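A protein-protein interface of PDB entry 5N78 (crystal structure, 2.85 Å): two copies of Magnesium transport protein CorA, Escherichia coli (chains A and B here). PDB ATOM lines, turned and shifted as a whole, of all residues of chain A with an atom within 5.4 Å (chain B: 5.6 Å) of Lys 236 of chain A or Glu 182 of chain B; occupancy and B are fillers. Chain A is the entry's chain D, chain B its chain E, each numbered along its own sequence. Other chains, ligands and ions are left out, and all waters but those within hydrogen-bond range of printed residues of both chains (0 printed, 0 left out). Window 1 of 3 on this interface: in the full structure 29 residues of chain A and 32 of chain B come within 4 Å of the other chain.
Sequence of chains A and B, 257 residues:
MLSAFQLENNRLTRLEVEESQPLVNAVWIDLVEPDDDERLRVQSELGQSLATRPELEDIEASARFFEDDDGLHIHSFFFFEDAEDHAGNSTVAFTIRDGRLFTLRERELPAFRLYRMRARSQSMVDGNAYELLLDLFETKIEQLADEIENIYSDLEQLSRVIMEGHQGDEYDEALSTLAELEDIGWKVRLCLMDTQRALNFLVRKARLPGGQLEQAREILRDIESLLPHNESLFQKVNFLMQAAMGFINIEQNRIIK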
ATOM      1  N   LEU A 155     -39.466  25.686  -8.105  1.00  0.00           N
ATOM      2  CA  LEU A 155     -38.272  26.445  -8.381  1.00  0.00           C
ATOM      3  C   LEU A 155     -38.075  26.583  -9.886  1.00  0.00           C
ATOM      4  O   LEU A 155     -37.564  27.581 -10.365  1.00  0.00           O
ATOM      5  CB  LEU A 155     -37.090  25.714  -7.765  1.00  0.00           C
ATOM      6  CG  LEU A 155     -35.886  26.492  -7.292  1.00  0.00           C
ATOM      7  CD1 LEU A 155     -36.300  27.577  -6.316  1.00  0.00           C
ATOM      8  CD2 LEU A 155     -34.941  25.538  -6.600  1.00  0.00           C
ATOM      9  N   SER A 159     -37.983  30.135 -11.476  1.00  0.00           N
ATOM     10  CA  SER A 159     -36.831  30.523 -12.266  1.00  0.00           C
ATOM     11  C   SER A 159     -37.230  31.303 -13.514  1.00  0.00           C
ATOM     12  O   SER A 159     -36.605  32.288 -13.854  1.00  0.00           O
ATOM     13  CB  SER A 159     -36.020  29.319 -12.680  1.00  0.00           C
ATOM     14  OG  SER A 159     -34.842  29.758 -13.343  1.00  0.00           O
ATOM     15  N   SER A 232     -28.410  20.878  -3.307  1.00  0.00           N
ATOM     16  CA  SER A 232     -28.512  21.357  -4.649  1.00  0.00           C
ATOM     17  C   SER A 232     -29.525  22.475  -4.754  1.00  0.00           C
ATOM     18  O   SER A 232     -29.306  23.455  -5.460  1.00  0.00           O
ATOM     19  CB  SER A 232     -28.928  20.206  -5.547  1.00  0.00           C
ATOM     20  OG  SER A 232     -28.599  20.490  -6.882  1.00  0.00           O
ATOM     21  N   LEU A 233     -30.638  22.335  -4.051  1.00  0.00           N
ATOM     22  CA  LEU A 233     -31.668  23.363  -4.042  1.00  0.00           C
ATOM     23  C   LEU A 233     -31.215  24.640  -3.366  1.00  0.00           C
ATOM     24  O   LEU A 233     -31.549  25.713  -3.839  1.00  0.00           O
ATOM     25  CB  LEU A 233     -32.925  22.851  -3.380  1.00  0.00           C
ATOM     26  CG  LEU A 233     -33.567  21.644  -4.067  1.00  0.00           C
ATOM     27  CD1 LEU A 233     -34.723  21.154  -3.225  1.00  0.00           C
ATOM     28  CD2 LEU A 233     -34.055  21.952  -5.458  1.00  0.00           C
ATOM     29  N   PHE A 234     -30.421  24.557  -2.309  1.00  0.00           N
ATOM     30  CA  PHE A 234     -29.920  25.786  -1.682  1.00  0.00           C
ATOM     31  C   PHE A 234     -29.039  26.569  -2.641  1.00  0.00           C
ATOM     32  O   PHE A 234     -29.171  27.783  -2.714  1.00  0.00           O
ATOM     33  CB  PHE A 234     -29.184  25.541  -0.361  1.00  0.00           C
ATOM     34  CG  PHE A 234     -30.081  25.038   0.724  1.00  0.00           C
ATOM     35  CD1 PHE A 234     -31.144  25.833   1.177  1.00  0.00           C
ATOM     36  CD2 PHE A 234     -29.920  23.752   1.256  1.00  0.00           C
ATOM     37  CE1 PHE A 234     -32.019  25.359   2.158  1.00  0.00           C
ATOM     38  CE2 PHE A 234     -30.789  23.273   2.229  1.00  0.00           C
ATOM     39  CZ  PHE A 234     -31.837  24.076   2.682  1.00  0.00           C
ATOM     40  N   GLN A 235     -28.166  25.901  -3.386  1.00  0.00           N
ATOM     41  CA  GLN A 235     -27.332  26.611  -4.346  1.00  0.00           C
ATOM     42  C   GLN A 235     -28.155  27.388  -5.346  1.00  0.00           C
ATOM     43  O   GLN A 235     -27.770  28.478  -5.750  1.00  0.00           O
ATOM     44  CB  GLN A 235     -26.502  25.653  -5.156  1.00  0.00           C
ATOM     45  CG  GLN A 235     -25.381  24.979  -4.401  1.00  0.00           C
ATOM     46  CD  GLN A 235     -24.263  24.592  -5.332  1.00  0.00           C
ATOM     47  OE1 GLN A 235     -24.377  24.749  -6.564  1.00  0.00           O
ATOM     48  NE2 GLN A 235     -23.166  24.101  -4.763  1.00  0.00           N
ATOM     49  N   LYS A 236     -29.258  26.782  -5.790  1.00  0.00           N
ATOM     50  CA  LYS A 236     -30.127  27.372  -6.810  1.00  0.00           C
ATOM     51  C   LYS A 236     -30.850  28.550  -6.225  1.00  0.00           C
ATOM     52  O   LYS A 236     -30.867  29.639  -6.786  1.00  0.00           O
ATOM     53  CB  LYS A 236     -31.153  26.356  -7.297  1.00  0.00           C
ATOM     54  CG  LYS A 236     -31.977  26.802  -8.496  1.00  0.00           C
ATOM     55  CD  LYS A 236     -31.138  26.925  -9.748  1.00  0.00           C
ATOM     56  CE  LYS A 236     -32.023  27.130 -10.964  1.00  0.00           C
ATOM     57  NZ  LYS A 236     -31.242  27.318 -12.225  1.00  0.00           N
ATOM     58  N   VAL A 237     -31.449  28.310  -5.084  1.00  0.00           N
ATOM     59  CA  VAL A 237     -32.150  29.340  -4.396  1.00  0.00           C
ATOM     60  C   VAL A 237     -31.267  30.546  -4.148  1.00  0.00           C
ATOM     61  O   VAL A 237     -31.734  31.673  -4.330  1.00  0.00           O
ATOM     62  CB  VAL A 237     -32.726  28.812  -3.106  1.00  0.00           C
ATOM     63  CG1 VAL A 237     -33.092  29.943  -2.159  1.00  0.00           C
ATOM     64  CG2 VAL A 237     -33.957  27.996  -3.444  1.00  0.00           C
ATOM     65  N   ASN A 238     -30.032  30.330  -3.706  1.00  0.00           N
ATOM     66  CA  ASN A 238     -29.145  31.460  -3.434  1.00  0.00           C
ATOM     67  C   ASN A 238     -28.762  32.224  -4.677  1.00  0.00           C
ATOM     68  O   ASN A 238     -28.655  33.452  -4.660  1.00  0.00           O
ATOM     69  CB  ASN A 238     -27.880  31.037  -2.679  1.00  0.00           C
ATOM     70  CG  ASN A 238     -28.158  30.709  -1.225  1.00  0.00           C
ATOM     71  OD1 ASN A 238     -28.974  31.356  -0.579  1.00  0.00           O
ATOM     72  ND2 ASN A 238     -27.536  29.663  -0.729  1.00  0.00           N
ATOM     73  N   PHE A 239     -28.576  31.491  -5.759  1.00  0.00           N
ATOM     74  CA  PHE A 239     -28.263  32.114  -6.992  1.00  0.00           C
ATOM     75  C   PHE A 239     -29.436  32.957  -7.470  1.00  0.00           C
ATOM     76  O   PHE A 239     -29.239  34.046  -7.979  1.00  0.00           O
ATOM     77  CB  PHE A 239     -27.938  31.082  -8.031  1.00  0.00           C
ATOM     78  CG  PHE A 239     -27.708  31.667  -9.362  1.00  0.00           C
ATOM     79  CD1 PHE A 239     -26.543  32.348  -9.630  1.00  0.00           C
ATOM     80  CD2 PHE A 239     -28.681  31.609 -10.336  1.00  0.00           C
ATOM     81  CE1 PHE A 239     -26.321  32.926 -10.859  1.00  0.00           C
ATOM     82  CE2 PHE A 239     -28.468  32.190 -11.578  1.00  0.00           C
ATOM     83  CZ  PHE A 239     -27.286  32.851 -11.840  1.00  0.00           C
ATOM     84  N   LEU A 240     -30.645  32.434  -7.375  1.00  0.00           N
ATOM     85  CA  LEU A 240     -31.817  33.143  -7.869  1.00  0.00           C
ATOM     86  C   LEU A 240     -32.041  34.422  -7.097  1.00  0.00           C
ATOM     87  O   LEU A 240     -32.384  35.451  -7.672  1.00  0.00           O
ATOM     88  CB  LEU A 240     -33.052  32.269  -7.769  1.00  0.00           C
ATOM     89  CG  LEU A 240     -33.496  31.530  -9.038  1.00  0.00           C
ATOM     90  CD1 LEU A 240     -32.418  30.639  -9.570  1.00  0.00           C
ATOM     91  CD2 LEU A 240     -34.694  30.668  -8.693  1.00  0.00           C
ATOM     92  N   MET A 241     -31.805  34.353  -5.800  1.00  0.00           N
ATOM     93  CA  MET A 241     -31.839  35.509  -4.944  1.00  0.00           C
ATOM     94  C   MET A 241     -30.896  36.563  -5.502  1.00  0.00           C
ATOM     95  O   MET A 241     -31.280  37.687  -5.754  1.00  0.00           O
ATOM     96  CB  MET A 241     -31.430  35.075  -3.542  1.00  0.00           C
ATOM     97  CG  MET A 241     -31.439  36.135  -2.471  1.00  0.00           C
ATOM     98  SD  MET A 241     -33.045  36.902  -2.233  1.00  0.00           S
ATOM     99  CE  MET A 241     -33.918  35.488  -1.591  1.00  0.00           C
ATOM    100  N   THR B 177     -28.591  35.628 -19.678  1.00  0.00           N
ATOM    101  CA  THR B 177     -27.691  34.613 -20.206  1.00  0.00           C
ATOM    102  C   THR B 177     -27.009  33.875 -19.067  1.00  0.00           C
ATOM    103  O   THR B 177     -27.011  32.659 -19.038  1.00  0.00           O
ATOM    104  CB  THR B 177     -26.622  35.196 -21.142  1.00  0.00           C
ATOM    105  OG1 THR B 177     -27.240  36.029 -22.128  1.00  0.00           O
ATOM    106  CG2 THR B 177     -25.893  34.096 -21.857  1.00  0.00           C
ATOM    107  N   LEU B 178     -26.400  34.603 -18.147  1.00  0.00           N
ATOM    108  CA  LEU B 178     -25.827  33.987 -16.966  1.00  0.00           C
ATOM    109  C   LEU B 178     -26.772  33.010 -16.297  1.00  0.00           C
ATOM    110  O   LEU B 178     -26.384  31.904 -15.966  1.00  0.00           O
ATOM    111  CB  LEU B 178     -25.522  35.023 -15.914  1.00  0.00           C
ATOM    112  CG  LEU B 178     -24.117  35.507 -15.771  1.00  0.00           C
ATOM    113  CD1 LEU B 178     -24.084  36.289 -14.472  1.00  0.00           C
ATOM    114  CD2 LEU B 178     -23.136  34.359 -15.695  1.00  0.00           C
ATOM    115  N   ALA B 179     -27.999  33.449 -16.050  1.00  0.00           N
ATOM    116  CA  ALA B 179     -28.988  32.601 -15.418  1.00  0.00           C
ATOM    117  C   ALA B 179     -29.327  31.357 -16.249  1.00  0.00           C
ATOM    118  O   ALA B 179     -29.621  30.322 -15.694  1.00  0.00           O
ATOM    119  CB  ALA B 179     -30.234  33.390 -15.166  1.00  0.00           C
ATOM    120  N   GLU B 180     -29.299  31.461 -17.576  1.00  0.00           N
ATOM    121  CA  GLU B 180     -29.542  30.320 -18.444  1.00  0.00           C
ATOM    122  C   GLU B 180     -28.359  29.322 -18.351  1.00  0.00           C
ATOM    123  O   GLU B 180     -28.541  28.113 -18.307  1.00  0.00           O
ATOM    124  CB  GLU B 180     -29.745  30.837 -19.861  1.00  0.00           C
ATOM    125  CG  GLU B 180     -30.166  29.789 -20.910  1.00  0.00           C
ATOM    126  CD  GLU B 180     -29.629  30.096 -22.333  1.00  0.00           C
ATOM    127  OE1 GLU B 180     -29.473  31.302 -22.691  1.00  0.00           O
ATOM    128  OE2 GLU B 180     -29.337  29.124 -23.098  1.00  0.00           O
ATOM    129  N   LEU B 181     -27.139  29.837 -18.308  1.00  0.00           N
ATOM    130  CA  LEU B 181     -25.961  28.996 -18.182  1.00  0.00           C
ATOM    131  C   LEU B 181     -25.868  28.305 -16.806  1.00  0.00           C
ATOM    132  O   LEU B 181     -25.416  27.169 -16.711  1.00  0.00           O
ATOM    133  CB  LEU B 181     -24.681  29.802 -18.478  1.00  0.00           C
ATOM    134  CG  LEU B 181     -24.585  30.307 -19.919  1.00  0.00           C
ATOM    135  CD1 LEU B 181     -23.347  31.157 -20.183  1.00  0.00           C
ATOM    136  CD2 LEU B 181     -24.613  29.149 -20.901  1.00  0.00           C
ATOM    137  N   GLU B 182     -26.282  28.995 -15.752  1.00  0.00           N
ATOM    138  CA  GLU B 182     -26.273  28.396 -14.435  1.00  0.00           C
ATOM    139  C   GLU B 182     -27.233  27.232 -14.484  1.00  0.00           C
ATOM    140  O   GLU B 182     -26.906  26.133 -14.054  1.00  0.00           O
ATOM    141  CB  GLU B 182     -26.702  29.386 -13.359  1.00  0.00           C
ATOM    142  CG  GLU B 182     -26.482  28.919 -11.929  1.00  0.00           C
ATOM    143  CD  GLU B 182     -27.659  28.144 -11.330  1.00  0.00           C
ATOM    144  OE1 GLU B 182     -28.731  28.066 -11.979  1.00  0.00           O
ATOM    145  OE2 GLU B 182     -27.505  27.577 -10.202  1.00  0.00           O
ATOM    146  N   ASP B 183     -28.408  27.459 -15.047  1.00  0.00           N
ATOM    147  CA  ASP B 183     -29.414  26.418 -15.086  1.00  0.00           C
ATOM    148  C   ASP B 183     -28.993  25.159 -15.849  1.00  0.00           C
ATOM    149  O   ASP B 183     -29.351  24.067 -15.473  1.00  0.00           O
ATOM    150  CB  ASP B 183     -30.662  26.957 -15.722  1.00  0.00           C
ATOM    151  CG  ASP B 183     -31.825  26.029 -15.579  1.00  0.00           C
ATOM    152  OD1 ASP B 183     -32.189  25.740 -14.400  1.00  0.00           O
ATOM    153  OD2 ASP B 183     -32.372  25.618 -16.650  1.00  0.00           O
ATOM    154  N   ILE B 184     -28.282  25.322 -16.953  1.00  0.00           N
ATOM    155  CA  ILE B 184     -27.829  24.183 -17.713  1.00  0.00           C
ATOM    156  C   ILE B 184     -26.827  23.433 -16.859  1.00  0.00           C
ATOM    157  O   ILE B 184     -26.935  22.237 -16.684  1.00  0.00           O
ATOM    158  CB  ILE B 184     -27.201  24.621 -19.034  1.00  0.00           C
ATOM    159  CG1 ILE B 184     -28.288  25.129 -19.968  1.00  0.00           C
ATOM    160  CG2 ILE B 184     -26.548  23.457 -19.732  1.00  0.00           C
ATOM    161  CD1 ILE B 184     -27.768  26.029 -21.057  1.00  0.00           C
ATOM    162  N   GLY B 185     -25.851  24.142 -16.306  1.00  0.00           N
ATOM    163  CA  GLY B 185     -24.834  23.499 -15.497  1.00  0.00           C
ATOM    164  C   GLY B 185     -25.441  22.728 -14.354  1.00  0.00           C
ATOM    165  O   GLY B 185     -25.059  21.599 -14.059  1.00  0.00           O
ATOM    166  N   TRP B 186     -26.444  23.332 -13.748  1.00  0.00           N
ATOM    167  CA  TRP B 186     -27.155  22.737 -12.628  1.00  0.00           C
ATOM    168  C   TRP B 186     -27.808  21.451 -13.062  1.00  0.00           C
ATOM    169  O   TRP B 186     -27.651  20.462 -12.421  1.00  0.00           O
ATOM    170  CB  TRP B 186     -28.216  23.716 -12.156  1.00  0.00           C
ATOM    171  CG  TRP B 186     -28.870  23.402 -10.896  1.00  0.00           C
ATOM    172  CD1 TRP B 186     -28.302  23.331  -9.672  1.00  0.00           C
ATOM    173  CD2 TRP B 186     -30.259  23.175 -10.719  1.00  0.00           C
ATOM    174  NE1 TRP B 186     -29.256  23.039  -8.730  1.00  0.00           N
ATOM    175  CE2 TRP B 186     -30.467  22.934  -9.358  1.00  0.00           C
ATOM    176  CE3 TRP B 186     -31.356  23.154 -11.591  1.00  0.00           C
ATOM    177  CZ2 TRP B 186     -31.712  22.694  -8.842  1.00  0.00           C
ATOM    178  CZ3 TRP B 186     -32.595  22.892 -11.080  1.00  0.00           C
ATOM    179  CH2 TRP B 186     -32.767  22.678  -9.718  1.00  0.00           C
ATOM    180  N   LYS B 187     -28.516  21.472 -14.178  1.00  0.00           N
ATOM    181  CA  LYS B 187     -29.157  20.286 -14.693  1.00  0.00           C
ATOM    182  C   LYS B 187     -28.175  19.254 -15.171  1.00  0.00           C
ATOM    183  O   LYS B 187     -28.392  18.069 -14.971  1.00  0.00           O
ATOM    184  CB  LYS B 187     -30.158  20.648 -15.776  1.00  0.00           C
ATOM    185  CG  LYS B 187     -31.454  21.096 -15.123  1.00  0.00           C
ATOM    186  CD  LYS B 187     -32.271  22.010 -15.985  1.00  0.00           C
ATOM    187  CE  LYS B 187     -33.409  22.585 -15.171  1.00  0.00           C
ATOM    188  NZ  LYS B 187     -34.256  23.465 -16.037  1.00  0.00           N
ATOM    189  N   PHE B 234     -19.785  27.006 -11.774  1.00  0.00           N
ATOM    190  CA  PHE B 234     -20.647  27.632 -10.799  1.00  0.00           C
ATOM    191  C   PHE B 234     -19.836  28.784 -10.080  1.00  0.00           C
ATOM    192  O   PHE B 234     -20.331  29.897  -9.939  1.00  0.00           O
ATOM    193  CB  PHE B 234     -21.244  26.504  -9.876  1.00  0.00           C
ATOM    194  CG  PHE B 234     -22.405  26.941  -9.103  1.00  0.00           C
ATOM    195  CD1 PHE B 234     -23.558  27.384  -9.753  1.00  0.00           C
ATOM    196  CD2 PHE B 234     -22.351  26.961  -7.704  1.00  0.00           C
ATOM    197  CE1 PHE B 234     -24.646  27.842  -9.007  1.00  0.00           C
ATOM    198  CE2 PHE B 234     -23.432  27.399  -6.961  1.00  0.00           C
ATOM    199  CZ  PHE B 234     -24.585  27.837  -7.617  1.00  0.00           C
ATOM    200  N   VAL B 237     -19.686  31.675 -12.702  1.00  0.00           N
ATOM    201  CA  VAL B 237     -20.988  32.250 -12.815  1.00  0.00           C
ATOM    202  C   VAL B 237     -21.370  33.113 -11.633  1.00  0.00           C
ATOM    203  O   VAL B 237     -21.879  34.211 -11.819  1.00  0.00           O
ATOM    204  CB  VAL B 237     -22.028  31.162 -13.019  1.00  0.00           C
ATOM    205  CG1 VAL B 237     -23.424  31.683 -12.713  1.00  0.00           C
ATOM    206  CG2 VAL B 237     -21.948  30.680 -14.459  1.00  0.00           C
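The side-chain amino group (NZ) of Lys 236 of chain A lies within salt-bridge range of the side-chain carboxylate (OD1) of Asp 183 of chain B, at 2.8 Å. The side-chain hydroxyl of Ser 232 of chain A lies within hydrogen-bond range of the indole nitrogen of Trp 186 of chain B (3.2 Å). The side-chain amino group of Lys 236 of chain A lies within salt-bridge range of the side-chain carboxylate of Glu 182 of chain B (2.6 Å).
NZ of Lys 187 of chain B lies within salt-bridge range of OD2 of Asp 183 of chain B, at 2.9 Å.
Phe 234 of chain B touches Gln 235 of chain A (CE2 to OE1, 2.8 Å). CD of Lys 236 of chain A touches CD2 of Trp 186 of chain B, at 3.97 Å. CE2 of Phe 239 of chain A touches CA of Ala 179 of chain B, 3.9 Å away. Glu 182 of chain B touches Phe 239 of chain A. Val 237 of chain B touches Phe 239 of chain A.
Printed residues of chain B within 4 Å of Ser 232 of chain A: Trp 186. Lys 236 of chain A touches just these residues of chain B: Glu 182 (2.6 Å), Asp 183 (2.8 Å) and Trp 186 (3.97 Å). Printed residues of chain A within 4 Å of Ala 179 of chain B: Phe 239. Glu 182 of chain B touches just these residues of chain A: Lys 236 (2.6 Å) and Phe 239 (3.7 Å). Printed residues of chain A within 4 Å of Val 237 of chain B: Phe 239. The nearest residue of chain A that does not touch Glu 182 of chain B is Gln 235 of chain A (4.5 Å). The nearest printed residue of chain B that does not touch Phe 239 of chain A is Leu 178 of chain B (4.3 Å).
Of the 12 printed residues of chain A, 4 touch a printed residue of chain B. Hydrophobic or aromatic side chains of chain A within 4 Å of the printed part of chain B: Phe 239. Of the 13 printed residues of chain B, 6 touch a printed residue of chain A. Hydrophobic or aromatic side chains of chain B within 4 Å of the printed part of chain A: Trp 186, Phe 234 and Val 237. Among the printed residues, Asp or Glu carboxylates within 4 Å of a Lys or Arg side-chain nitrogen of the other chain: Lys 236 of chain A with Glu 182 of chain B (2.6 Å) and Lys 236 of chain A with Asp 183 of chain B (2.8 Å).
Positions printed for both chains: 234 and 237.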
